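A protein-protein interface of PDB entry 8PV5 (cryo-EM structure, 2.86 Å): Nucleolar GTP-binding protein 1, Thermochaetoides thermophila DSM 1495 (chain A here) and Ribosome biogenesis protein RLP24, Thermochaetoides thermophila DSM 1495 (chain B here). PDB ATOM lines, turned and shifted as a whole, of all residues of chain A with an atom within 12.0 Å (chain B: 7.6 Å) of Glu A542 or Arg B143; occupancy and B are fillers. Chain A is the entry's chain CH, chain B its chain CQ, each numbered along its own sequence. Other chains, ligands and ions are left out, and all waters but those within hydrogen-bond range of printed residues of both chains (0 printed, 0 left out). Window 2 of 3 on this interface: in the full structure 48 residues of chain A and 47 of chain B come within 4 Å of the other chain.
Gln A536 touches Arg B138 (CG to NH2, 3.4 Å). N of Gly B139 touches CA of Gly A538 (3.7 Å).
The side-chain hydroxyl of Thr A541 is in hydrogen-bond range of the side-chain carboxylate of Glu A542, 3.5 Å away. NE2 of Gln A536 lies within hydrogen-bond range of OD1 of Asp A532 (3.3 Å).
The side-chain carboxylate of Asp A532 is in salt-bridge range of the guanidinium group of Arg B138 (2.5 Å). The side-chain carboxylate of Asp A535 lies within hydrogen-bond range of the backbone NH of Ser B140 (3.1 Å). The guanidinium group (NH1) of Arg B143 is in salt-bridge range of the side-chain carboxylate (OE2) of Glu A542 (3.1 Å). The side-chain carboxylate of Asp A535 sits at hydrogen-bond distance from the backbone NH of Gly B139, 3.1 Å away. The guanidinium group of Arg B138 lies within salt-bridge range of the side-chain carboxylate of Asp A535, at 3.99 Å.
Of the 13 printed residues of chain B, 4 touch a printed residue of chain A. Printed residues of chain B that touch a printed residue of chain A: Arg B138, Gly B139, Ser B140 and Arg B143. Along chain B the printed residues that touch a printed residue of chain A span positions 138 to 143. Among the printed residues, Asp or Glu carboxylates within 4 Å of a Lys or Arg side-chain nitrogen of the other chain: Asp A532 with Arg B138 (2.5 Å), Asp A535 with Arg B138 (3.99 Å) and Glu A542 with Arg B143 (3.1 Å).
Glu A531 touches none of the printed residues of chain B. Of the printed residues of chain B, Asp A532 touches Arg B138 (2.5 Å). Of the printed residues of chain B, Asp A535 touches Arg B138, Gly B139 and Ser B140. Of the printed residues of chain B, Gln A536 touches Arg B138. Printed residues of chain B within 4 Å of Gly A538: Gly B139. Glu A542 touches just one residue of chain B: Arg B143. Leu A546 touches none of the printed residues of chain B. Of the printed residues of chain A, Arg B138 touches Asp A532, Asp A535 and Gln A536. Printed residues of chain A within 4 Å of Gly B139: Asp A535 (3.1 Å) and Gly A538 (3.7 Å). No residue of chain A comes within 4 Å of Glu B141. No residue of chain A comes within 4 Å of Lys B142. Of chain A, only Glu A542 (3.1 Å) comes within 4 Å of Arg B143. No residue of chain A comes within 4 Å of Leu B145. No residue of chain A comes within 4 Å of Glu B147. The nearest residue of chain B that does not touch Glu A542 is Ser B140 (4.8 Å). The nearest residue of chain A that does not touch Arg B143 is Ala A543 (4.4 Å).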
ATOM      1  N   LEU A 527       4.930 -19.633  12.129  1.00  0.00           N
ATOM      2  CA  LEU A 527       4.094 -18.700  11.380  1.00  0.00           C
ATOM      3  C   LEU A 527       3.695 -19.270  10.027  1.00  0.00           C
ATOM      4  O   LEU A 527       2.555 -19.093   9.589  1.00  0.00           O
ATOM      5  CB  LEU A 527       4.822 -17.368  11.200  1.00  0.00           C
ATOM      6  CG  LEU A 527       4.041 -16.274  10.469  1.00  0.00           C
ATOM      7  CD1 LEU A 527       2.737 -15.963  11.188  1.00  0.00           C
ATOM      8  CD2 LEU A 527       4.882 -15.019  10.304  1.00  0.00           C
ATOM      9  N   SER A 528       4.620 -19.959   9.352  1.00  0.00           N
ATOM     10  CA  SER A 528       4.314 -20.552   8.053  1.00  0.00           C
ATOM     11  C   SER A 528       3.261 -21.646   8.180  1.00  0.00           C
ATOM     12  O   SER A 528       2.347 -21.744   7.351  1.00  0.00           O
ATOM     13  CB  SER A 528       5.591 -21.101   7.416  1.00  0.00           C
ATOM     14  OG  SER A 528       6.126 -22.163   8.184  1.00  0.00           O
ATOM     15  N   LEU A 530       0.970 -21.935  10.621  1.00  0.00           N
ATOM     16  CA  LEU A 530      -0.315 -21.329  10.969  1.00  0.00           C
ATOM     17  C   LEU A 530      -0.921 -20.617   9.763  1.00  0.00           C
ATOM     18  O   LEU A 530      -2.143 -20.629   9.567  1.00  0.00           O
ATOM     19  CB  LEU A 530      -0.134 -20.382  12.162  1.00  0.00           C
ATOM     20  CG  LEU A 530      -1.316 -19.721  12.882  1.00  0.00           C
ATOM     21  CD1 LEU A 530      -0.917 -19.434  14.313  1.00  0.00           C
ATOM     22  CD2 LEU A 530      -1.740 -18.420  12.234  1.00  0.00           C
ATOM     23  N   GLU A 531      -0.069 -20.003   8.938  1.00  0.00           N
ATOM     24  CA  GLU A 531      -0.509 -19.390   7.690  1.00  0.00           C
ATOM     25  C   GLU A 531      -1.135 -20.422   6.762  1.00  0.00           C
ATOM     26  O   GLU A 531      -2.209 -20.192   6.195  1.00  0.00           O
ATOM     27  CB  GLU A 531       0.686 -18.717   7.013  1.00  0.00           C
ATOM     28  CG  GLU A 531       0.406 -18.147   5.641  1.00  0.00           C
ATOM     29  CD  GLU A 531      -0.463 -16.917   5.697  1.00  0.00           C
ATOM     30  OE1 GLU A 531      -0.416 -16.205   6.722  1.00  0.00           O
ATOM     31  OE2 GLU A 531      -1.196 -16.664   4.718  1.00  0.00           O
ATOM     32  N   ASP A 532      -0.480 -21.578   6.614  1.00  0.00           N
ATOM     33  CA  ASP A 532      -1.001 -22.630   5.746  1.00  0.00           C
ATOM     34  C   ASP A 532      -2.317 -23.185   6.281  1.00  0.00           C
ATOM     35  O   ASP A 532      -3.247 -23.449   5.512  1.00  0.00           O
ATOM     36  CB  ASP A 532       0.039 -23.742   5.595  1.00  0.00           C
ATOM     37  CG  ASP A 532      -0.137 -24.548   4.315  1.00  0.00           C
ATOM     38  OD1 ASP A 532      -1.255 -24.583   3.759  1.00  0.00           O
ATOM     39  OD2 ASP A 532       0.858 -25.146   3.857  1.00  0.00           O
ATOM     40  N   HIS A 533      -2.420 -23.352   7.603  1.00  0.00           N
ATOM     41  CA  HIS A 533      -3.651 -23.880   8.190  1.00  0.00           C
ATOM     42  C   HIS A 533      -4.816 -22.910   8.009  1.00  0.00           C
ATOM     43  O   HIS A 533      -5.920 -23.313   7.615  1.00  0.00           O
ATOM     44  CB  HIS A 533      -3.431 -24.192   9.670  1.00  0.00           C
ATOM     45  CG  HIS A 533      -4.633 -24.767  10.354  1.00  0.00           C
ATOM     46  ND1 HIS A 533      -4.914 -26.116  10.349  1.00  0.00           N
ATOM     47  CD2 HIS A 533      -5.627 -24.178  11.059  1.00  0.00           C
ATOM     48  CE1 HIS A 533      -6.026 -26.334  11.027  1.00  0.00           C
ATOM     49  NE2 HIS A 533      -6.479 -25.175  11.469  1.00  0.00           N
ATOM     50  N   LEU A 534      -4.585 -21.620   8.270  1.00  0.00           N
ATOM     51  CA  LEU A 534      -5.655 -20.642   8.094  1.00  0.00           C
ATOM     52  C   LEU A 534      -6.012 -20.475   6.622  1.00  0.00           C
ATOM     53  O   LEU A 534      -7.168 -20.195   6.285  1.00  0.00           O
ATOM     54  CB  LEU A 534      -5.260 -19.302   8.712  1.00  0.00           C
ATOM     55  CG  LEU A 534      -5.253 -19.238  10.244  1.00  0.00           C
ATOM     56  CD1 LEU A 534      -5.071 -17.807  10.716  1.00  0.00           C
ATOM     57  CD2 LEU A 534      -6.524 -19.841  10.826  1.00  0.00           C
ATOM     58  N   ASP A 535      -5.035 -20.659   5.729  1.00  0.00           N
ATOM     59  CA  ASP A 535      -5.321 -20.615   4.299  1.00  0.00           C
ATOM     60  C   ASP A 535      -6.190 -21.795   3.878  1.00  0.00           C
ATOM     61  O   ASP A 535      -7.136 -21.634   3.101  1.00  0.00           O
ATOM     62  CB  ASP A 535      -4.015 -20.593   3.507  1.00  0.00           C
ATOM     63  CG  ASP A 535      -4.073 -19.657   2.321  1.00  0.00           C
ATOM     64  OD1 ASP A 535      -3.022 -19.091   1.954  1.00  0.00           O
ATOM     65  OD2 ASP A 535      -5.172 -19.474   1.760  1.00  0.00           O
ATOM     66  N   GLN A 536      -5.885 -22.993   4.388  1.00  0.00           N
ATOM     67  CA  GLN A 536      -6.681 -24.167   4.041  1.00  0.00           C
ATOM     68  C   GLN A 536      -8.087 -24.113   4.618  1.00  0.00           C
ATOM     69  O   GLN A 536      -9.018 -24.624   3.987  1.00  0.00           O
ATOM     70  CB  GLN A 536      -5.985 -25.450   4.498  1.00  0.00           C
ATOM     71  CG  GLN A 536      -4.693 -25.754   3.765  1.00  0.00           C
ATOM     72  CD  GLN A 536      -4.031 -27.021   4.260  1.00  0.00           C
ATOM     73  OE1 GLN A 536      -4.504 -27.652   5.205  1.00  0.00           O
ATOM     74  NE2 GLN A 536      -2.926 -27.399   3.630  1.00  0.00           N
ATOM     75  N   LEU A 537      -8.272 -23.518   5.793  1.00  0.00           N
ATOM     76  CA  LEU A 537      -9.629 -23.258   6.268  1.00  0.00           C
ATOM     77  C   LEU A 537     -10.263 -22.021   5.641  1.00  0.00           C
ATOM     78  O   LEU A 537     -11.459 -21.792   5.842  1.00  0.00           O
ATOM     79  CB  LEU A 537      -9.684 -23.157   7.799  1.00  0.00           C
ATOM     80  CG  LEU A 537      -9.664 -24.454   8.625  1.00  0.00           C
ATOM     81  CD1 LEU A 537      -8.334 -25.180   8.642  1.00  0.00           C
ATOM     82  CD2 LEU A 537     -10.133 -24.174  10.050  1.00  0.00           C
ATOM     83  N   GLY A 538      -9.505 -21.229   4.886  1.00  0.00           N
ATOM     84  CA  GLY A 538     -10.112 -20.192   4.075  1.00  0.00           C
ATOM     85  C   GLY A 538     -10.240 -18.836   4.727  1.00  0.00           C
ATOM     86  O   GLY A 538     -11.258 -18.162   4.540  1.00  0.00           O
ATOM     87  N   VAL A 539      -9.234 -18.407   5.477  1.00  0.00           N
ATOM     88  CA  VAL A 539      -9.250 -17.117   6.156  1.00  0.00           C
ATOM     89  C   VAL A 539      -8.232 -16.206   5.487  1.00  0.00           C
ATOM     90  O   VAL A 539      -7.085 -16.605   5.252  1.00  0.00           O
ATOM     91  CB  VAL A 539      -8.951 -17.279   7.660  1.00  0.00           C
ATOM     92  CG1 VAL A 539      -8.879 -15.923   8.348  1.00  0.00           C
ATOM     93  CG2 VAL A 539     -10.004 -18.155   8.317  1.00  0.00           C
ATOM     94  N   ASP A 540      -8.652 -14.984   5.167  1.00  0.00           N
ATOM     95  CA  ASP A 540      -7.767 -13.995   4.553  1.00  0.00           C
ATOM     96  C   ASP A 540      -6.719 -13.519   5.562  1.00  0.00           C
ATOM     97  O   ASP A 540      -6.959 -12.632   6.384  1.00  0.00           O
ATOM     98  CB  ASP A 540      -8.592 -12.866   3.934  1.00  0.00           C
ATOM     99  CG  ASP A 540      -9.549 -12.192   4.918  1.00  0.00           C
ATOM    100  OD1 ASP A 540      -9.666 -12.634   6.080  1.00  0.00           O
ATOM    101  OD2 ASP A 540     -10.199 -11.204   4.515  1.00  0.00           O
ATOM    102  N   THR A 541      -5.526 -14.112   5.479  1.00  0.00           N
ATOM    103  CA  THR A 541      -4.494 -13.857   6.478  1.00  0.00           C
ATOM    104  C   THR A 541      -3.822 -12.507   6.266  1.00  0.00           C
ATOM    105  O   THR A 541      -3.402 -11.857   7.231  1.00  0.00           O
ATOM    106  CB  THR A 541      -3.453 -14.971   6.447  1.00  0.00           C
ATOM    107  OG1 THR A 541      -2.786 -14.959   5.180  1.00  0.00           O
ATOM    108  CG2 THR A 541      -4.110 -16.325   6.661  1.00  0.00           C
ATOM    109  N   GLU A 542      -3.687 -12.076   5.010  1.00  0.00           N
ATOM    110  CA  GLU A 542      -3.043 -10.793   4.745  1.00  0.00           C
ATOM    111  C   GLU A 542      -3.951  -9.631   5.130  1.00  0.00           C
ATOM    112  O   GLU A 542      -3.478  -8.505   5.328  1.00  0.00           O
ATOM    113  CB  GLU A 542      -2.628 -10.703   3.276  1.00  0.00           C
ATOM    114  CG  GLU A 542      -3.781 -10.689   2.287  1.00  0.00           C
ATOM    115  CD  GLU A 542      -4.166 -12.080   1.816  1.00  0.00           C
ATOM    116  OE1 GLU A 542      -3.747 -13.069   2.453  1.00  0.00           O
ATOM    117  OE2 GLU A 542      -4.885 -12.182   0.800  1.00  0.00           O
ATOM    118  N   ALA A 543      -5.256  -9.882   5.243  1.00  0.00           N
ATOM    119  CA  ALA A 543      -6.170  -8.854   5.720  1.00  0.00           C
ATOM    120  C   ALA A 543      -6.065  -8.639   7.224  1.00  0.00           C
ATOM    121  O   ALA A 543      -6.352  -7.535   7.699  1.00  0.00           O
ATOM    122  CB  ALA A 543      -7.609  -9.210   5.345  1.00  0.00           C
ATOM    123  N   ILE A 544      -5.664  -9.661   7.984  1.00  0.00           N
ATOM    124  CA  ILE A 544      -5.542  -9.535   9.434  1.00  0.00           C
ATOM    125  C   ILE A 544      -4.104  -9.327   9.891  1.00  0.00           C
ATOM    126  O   ILE A 544      -3.889  -8.916  11.043  1.00  0.00           O
ATOM    127  CB  ILE A 544      -6.152 -10.755  10.158  1.00  0.00           C
ATOM    128  CG1 ILE A 544      -5.393 -12.033   9.800  1.00  0.00           C
ATOM    129  CG2 ILE A 544      -7.625 -10.892   9.811  1.00  0.00           C
ATOM    130  CD1 ILE A 544      -5.951 -13.279  10.452  1.00  0.00           C
ATOM    131  N   GLY A 545      -3.117  -9.591   9.035  1.00  0.00           N
ATOM    132  CA  GLY A 545      -1.737  -9.273   9.352  1.00  0.00           C
ATOM    133  C   GLY A 545      -1.106 -10.137  10.424  1.00  0.00           C
ATOM    134  O   GLY A 545      -0.822  -9.657  11.527  1.00  0.00           O
ATOM    135  N   LEU A 546      -0.880 -11.416  10.116  1.00  0.00           N
ATOM    136  CA  LEU A 546      -0.263 -12.315  11.087  1.00  0.00           C
ATOM    137  C   LEU A 546       1.225 -12.034  11.260  1.00  0.00           C
ATOM    138  O   LEU A 546       1.817 -12.451  12.265  1.00  0.00           O
ATOM    139  CB  LEU A 546      -0.481 -13.766  10.662  1.00  0.00           C
ATOM    140  CG  LEU A 546      -1.933 -14.240  10.638  1.00  0.00           C
ATOM    141  CD1 LEU A 546      -2.048 -15.551   9.885  1.00  0.00           C
ATOM    142  CD2 LEU A 546      -2.472 -14.381  12.052  1.00  0.00           C
ATOM    143  N   ARG A 547       1.841 -11.343  10.296  1.00  0.00           N
ATOM    144  CA  ARG A 547       3.268 -11.038  10.378  1.00  0.00           C
ATOM    145  C   ARG A 547       3.575 -10.109  11.546  1.00  0.00           C
ATOM    146  O   ARG A 547       4.594 -10.271  12.227  1.00  0.00           O
ATOM    147  CB  ARG A 547       3.744 -10.418   9.064  1.00  0.00           C
ATOM    148  CG  ARG A 547       3.159 -11.067   7.821  1.00  0.00           C
ATOM    149  CD  ARG A 547       3.731 -12.455   7.591  1.00  0.00           C
ATOM    150  NE  ARG A 547       5.183 -12.429   7.452  1.00  0.00           N
ATOM    151  CZ  ARG A 547       5.920 -13.477   7.110  1.00  0.00           C
ATOM    152  NH1 ARG A 547       5.374 -14.655   6.859  1.00  0.00           N
ATOM    153  NH2 ARG A 547       7.240 -13.339   7.015  1.00  0.00           N
ATOM    154  N   ALA A 548       2.707  -9.125  11.787  1.00  0.00           N
ATOM    155  CA  ALA A 548       2.901  -8.230  12.923  1.00  0.00           C
ATOM    156  C   ALA A 548       2.623  -8.940  14.242  1.00  0.00           C
ATOM    157  O   ALA A 548       3.262  -8.644  15.258  1.00  0.00           O
ATOM    158  CB  ALA A 548       2.010  -6.996  12.777  1.00  0.00           C
ATOM    159  N   ARG A 549       1.671  -9.875  14.248  1.00  0.00           N
ATOM    160  CA  ARG A 549       1.351 -10.602  15.471  1.00  0.00           C
ATOM    161  C   ARG A 549       2.404 -11.644  15.820  1.00  0.00           C
ATOM    162  O   ARG A 549       2.517 -12.021  16.992  1.00  0.00           O
ATOM    163  CB  ARG A 549      -0.018 -11.271  15.345  1.00  0.00           C
ATOM    164  CG  ARG A 549      -1.122 -10.341  14.879  1.00  0.00           C
ATOM    165  CD  ARG A 549      -2.241 -11.114  14.186  1.00  0.00           C
ATOM    166  NE  ARG A 549      -3.428 -10.300  13.943  1.00  0.00           N
ATOM    167  CZ  ARG A 549      -4.274  -9.887  14.879  1.00  0.00           C
ATOM    168  NH1 ARG A 549      -4.134 -10.238  16.147  1.00  0.00           N
ATOM    169  NH2 ARG A 549      -5.298  -9.113  14.529  1.00  0.00           N
ATOM    170  N   ALA A 550       3.163 -12.125  14.840  1.00  0.00           N
ATOM    171  CA  ALA A 550       4.203 -13.106  15.118  1.00  0.00           C
ATOM    172  C   ALA A 550       5.366 -12.471  15.869  1.00  0.00           C
ATOM    173  O   ALA A 550       5.784 -11.349  15.570  1.00  0.00           O
ATOM    174  CB  ALA A 550       4.702 -13.733  13.817  1.00  0.00           C
ATOM    175  N   ARG B 138      -9.259 -21.813  -0.767  1.00  0.00           N
ATOM    176  CA  ARG B 138      -8.352 -21.110   0.126  1.00  0.00           C
ATOM    177  C   ARG B 138      -8.632 -19.611   0.112  1.00  0.00           C
ATOM    178  O   ARG B 138      -9.236 -19.082  -0.822  1.00  0.00           O
ATOM    179  CB  ARG B 138      -6.899 -21.374  -0.272  1.00  0.00           C
ATOM    180  CG  ARG B 138      -6.599 -22.821  -0.619  1.00  0.00           C
ATOM    181  CD  ARG B 138      -5.101 -23.046  -0.764  1.00  0.00           C
ATOM    182  NE  ARG B 138      -4.444 -23.203   0.528  1.00  0.00           N
ATOM    183  CZ  ARG B 138      -3.189 -23.603   0.686  1.00  0.00           C
ATOM    184  NH1 ARG B 138      -2.424 -23.904  -0.350  1.00  0.00           N
ATOM    185  NH2 ARG B 138      -2.691 -23.703   1.915  1.00  0.00           N
ATOM    186  N   GLY B 139      -8.194 -18.930   1.174  1.00  0.00           N
ATOM    187  CA  GLY B 139      -8.374 -17.488   1.244  1.00  0.00           C
ATOM    188  C   GLY B 139      -7.556 -16.742   0.205  1.00  0.00           C
ATOM    189  O   GLY B 139      -8.045 -15.799  -0.427  1.00  0.00           O
ATOM    190  N   SER B 140      -6.299 -17.153   0.016  1.00  0.00           N
ATOM    191  CA  SER B 140      -5.476 -16.569  -1.038  1.00  0.00           C
ATOM    192  C   SER B 140      -6.051 -16.879  -2.413  1.00  0.00           C
ATOM    193  O   SER B 140      -5.990 -16.044  -3.324  1.00  0.00           O
ATOM    194  CB  SER B 140      -4.041 -17.082  -0.930  1.00  0.00           C
ATOM    195  OG  SER B 140      -3.987 -18.483  -1.126  1.00  0.00           O
ATOM    196  N   GLU B 141      -6.623 -18.076  -2.573  1.00  0.00           N
ATOM    197  CA  GLU B 141      -7.295 -18.426  -3.819  1.00  0.00           C
ATOM    198  C   GLU B 141      -8.488 -17.515  -4.072  1.00  0.00           C
ATOM    199  O   GLU B 141      -8.687 -17.042  -5.193  1.00  0.00           O
ATOM    200  CB  GLU B 141      -7.731 -19.890  -3.789  1.00  0.00           C
ATOM    201  CG  GLU B 141      -7.741 -20.559  -5.154  1.00  0.00           C
ATOM    202  CD  GLU B 141      -6.357 -20.652  -5.764  1.00  0.00           C
ATOM    203  OE1 GLU B 141      -6.235 -20.462  -6.992  1.00  0.00           O
ATOM    204  OE2 GLU B 141      -5.391 -20.918  -5.019  1.00  0.00           O
ATOM    205  N   LYS B 142      -9.280 -17.237  -3.030  1.00  0.00           N
ATOM    206  CA  LYS B 142     -10.434 -16.353  -3.179  1.00  0.00           C
ATOM    207  C   LYS B 142     -10.008 -14.927  -3.507  1.00  0.00           C
ATOM    208  O   LYS B 142     -10.656 -14.250  -4.313  1.00  0.00           O
ATOM    209  CB  LYS B 142     -11.286 -16.372  -1.909  1.00  0.00           C
ATOM    210  CG  LYS B 142     -12.045 -17.667  -1.680  1.00  0.00           C
ATOM    211  CD  LYS B 142     -13.299 -17.430  -0.854  1.00  0.00           C
ATOM    212  CE  LYS B 142     -13.015 -17.552   0.633  1.00  0.00           C
ATOM    213  NZ  LYS B 142     -14.246 -17.876   1.406  1.00  0.00           N
ATOM    214  N   ARG B 143      -8.917 -14.457  -2.895  1.00  0.00           N
ATOM    215  CA  ARG B 143      -8.394 -13.130  -3.219  1.00  0.00           C
ATOM    216  C   ARG B 143      -7.908 -13.061  -4.665  1.00  0.00           C
ATOM    217  O   ARG B 143      -8.141 -12.064  -5.365  1.00  0.00           O
ATOM    218  CB  ARG B 143      -7.269 -12.761  -2.253  1.00  0.00           C
ATOM    219  CG  ARG B 143      -7.721 -12.550  -0.819  1.00  0.00           C
ATOM    220  CD  ARG B 143      -8.538 -11.272  -0.675  1.00  0.00           C
ATOM    221  NE  ARG B 143      -7.762 -10.094  -1.046  1.00  0.00           N
ATOM    222  CZ  ARG B 143      -6.987  -9.412  -0.213  1.00  0.00           C
ATOM    223  NH1 ARG B 143      -6.863  -9.759   1.057  1.00  0.00           N
ATOM    224  NH2 ARG B 143      -6.316  -8.358  -0.669  1.00  0.00           N
ATOM    225  N   ARG B 144      -7.232 -14.118  -5.132  1.00  0.00           N
ATOM    226  CA  ARG B 144      -6.744 -14.131  -6.508  1.00  0.00           C
ATOM    227  C   ARG B 144      -7.910 -14.200  -7.490  1.00  0.00           C
ATOM    228  O   ARG B 144      -7.880 -13.563  -8.549  1.00  0.00           O
ATOM    229  CB  ARG B 144      -5.767 -15.298  -6.705  1.00  0.00           C
ATOM    230  CG  ARG B 144      -5.003 -15.336  -8.043  1.00  0.00           C
ATOM    231  CD  ARG B 144      -5.677 -16.107  -9.176  1.00  0.00           C
ATOM    232  NE  ARG B 144      -5.875 -17.518  -8.874  1.00  0.00           N
ATOM    233  CZ  ARG B 144      -6.693 -18.316  -9.548  1.00  0.00           C
ATOM    234  NH1 ARG B 144      -7.365 -17.884 -10.602  1.00  0.00           N
ATOM    235  NH2 ARG B 144      -6.830 -19.581  -9.163  1.00  0.00           N
ATOM    236  N   LEU B 145      -8.959 -14.951  -7.143  1.00  0.00           N
ATOM    237  CA  LEU B 145     -10.154 -14.991  -7.981  1.00  0.00           C
ATOM    238  C   LEU B 145     -10.861 -13.642  -8.001  1.00  0.00           C
ATOM    239  O   LEU B 145     -11.404 -13.237  -9.033  1.00  0.00           O
ATOM    240  CB  LEU B 145     -11.114 -16.081  -7.501  1.00  0.00           C
ATOM    241  CG  LEU B 145     -10.664 -17.539  -7.613  1.00  0.00           C
ATOM    242  CD1 LEU B 145     -11.681 -18.472  -6.968  1.00  0.00           C
ATOM    243  CD2 LEU B 145     -10.373 -17.921  -9.035  1.00  0.00           C
ATOM    244  N   ALA B 146     -10.862 -12.931  -6.870  1.00  0.00           N
ATOM    245  CA  ALA B 146     -11.494 -11.615  -6.818  1.00  0.00           C
ATOM    246  C   ALA B 146     -10.747 -10.606  -7.684  1.00  0.00           C
ATOM    247  O   ALA B 146     -11.363  -9.840  -8.436  1.00  0.00           O
ATOM    248  CB  ALA B 146     -11.580 -11.130  -5.369  1.00  0.00           C
ATOM    249  N   GLU B 147      -9.411 -10.603  -7.611  1.00  0.00           N
ATOM    250  CA  GLU B 147      -8.657  -9.663  -8.439  1.00  0.00           C
ATOM    251  C   GLU B 147      -8.720 -10.054  -9.915  1.00  0.00           C
ATOM    252  O   GLU B 147      -8.744  -9.180 -10.790  1.00  0.00           O
ATOM    253  CB  GLU B 147      -7.209  -9.540  -7.950  1.00  0.00           C
ATOM    254  CG  GLU B 147      -6.376 -10.802  -7.974  1.00  0.00           C
ATOM    255  CD  GLU B 147      -5.642 -11.006  -9.289  1.00  0.00           C
ATOM    256  OE1 GLU B 147      -5.442 -10.019 -10.029  1.00  0.00           O
ATOM    257  OE2 GLU B 147      -5.266 -12.159  -9.585  1.00  0.00           O
ATOM    258  N   LEU B 148      -8.796 -11.357 -10.212  1.00  0.00           N
ATOM    259  CA  LEU B 148      -8.959 -11.791 -11.596  1.00  0.00           C
ATOM    260  C   LEU B 148     -10.327 -11.401 -12.145  1.00  0.00           C
ATOM    261  O   LEU B 148     -10.445 -11.011 -13.312  1.00  0.00           O
ATOM    262  CB  LEU B 148      -8.754 -13.302 -11.701  1.00  0.00           C
ATOM    263  CG  LEU B 148      -8.827 -13.923 -13.099  1.00  0.00           C
ATOM    264  CD1 LEU B 148      -7.724 -13.381 -13.998  1.00  0.00           C
ATOM    265  CD2 LEU B 148      -8.772 -15.439 -13.024  1.00  0.00           C
ATOM    266  N   ALA B 149     -11.374 -11.505 -11.321  1.00  0.00           N
ATOM    267  CA  ALA B 149     -12.703 -11.087 -11.753  1.00  0.00           C
ATOM    268  C   ALA B 149     -12.769  -9.579 -11.943  1.00  0.00           C
ATOM    269  O   ALA B 149     -13.433  -9.092 -12.863  1.00  0.00           O
ATOM    270  CB  ALA B 149     -13.754 -11.549 -10.744  1.00  0.00           C
ATOM    271  N   GLU B 160     -15.227 -19.213  -8.647  1.00  0.00           N
ATOM    272  CA  GLU B 160     -15.290 -20.126  -7.507  1.00  0.00           C
ATOM    273  C   GLU B 160     -15.719 -21.531  -7.913  1.00  0.00           C
ATOM    274  O   GLU B 160     -15.082 -22.503  -7.494  1.00  0.00           O
ATOM    275  CB  GLU B 160     -16.195 -19.605  -6.383  1.00  0.00           C
ATOM    276  CG  GLU B 160     -15.842 -18.242  -5.807  1.00  0.00           C
ATOM    277  CD  GLU B 160     -16.145 -18.130  -4.321  1.00  0.00           C
ATOM    278  OE1 GLU B 160     -15.779 -17.095  -3.711  1.00  0.00           O
ATOM    279  OE2 GLU B 160     -16.768 -19.067  -3.775  1.00  0.00           O
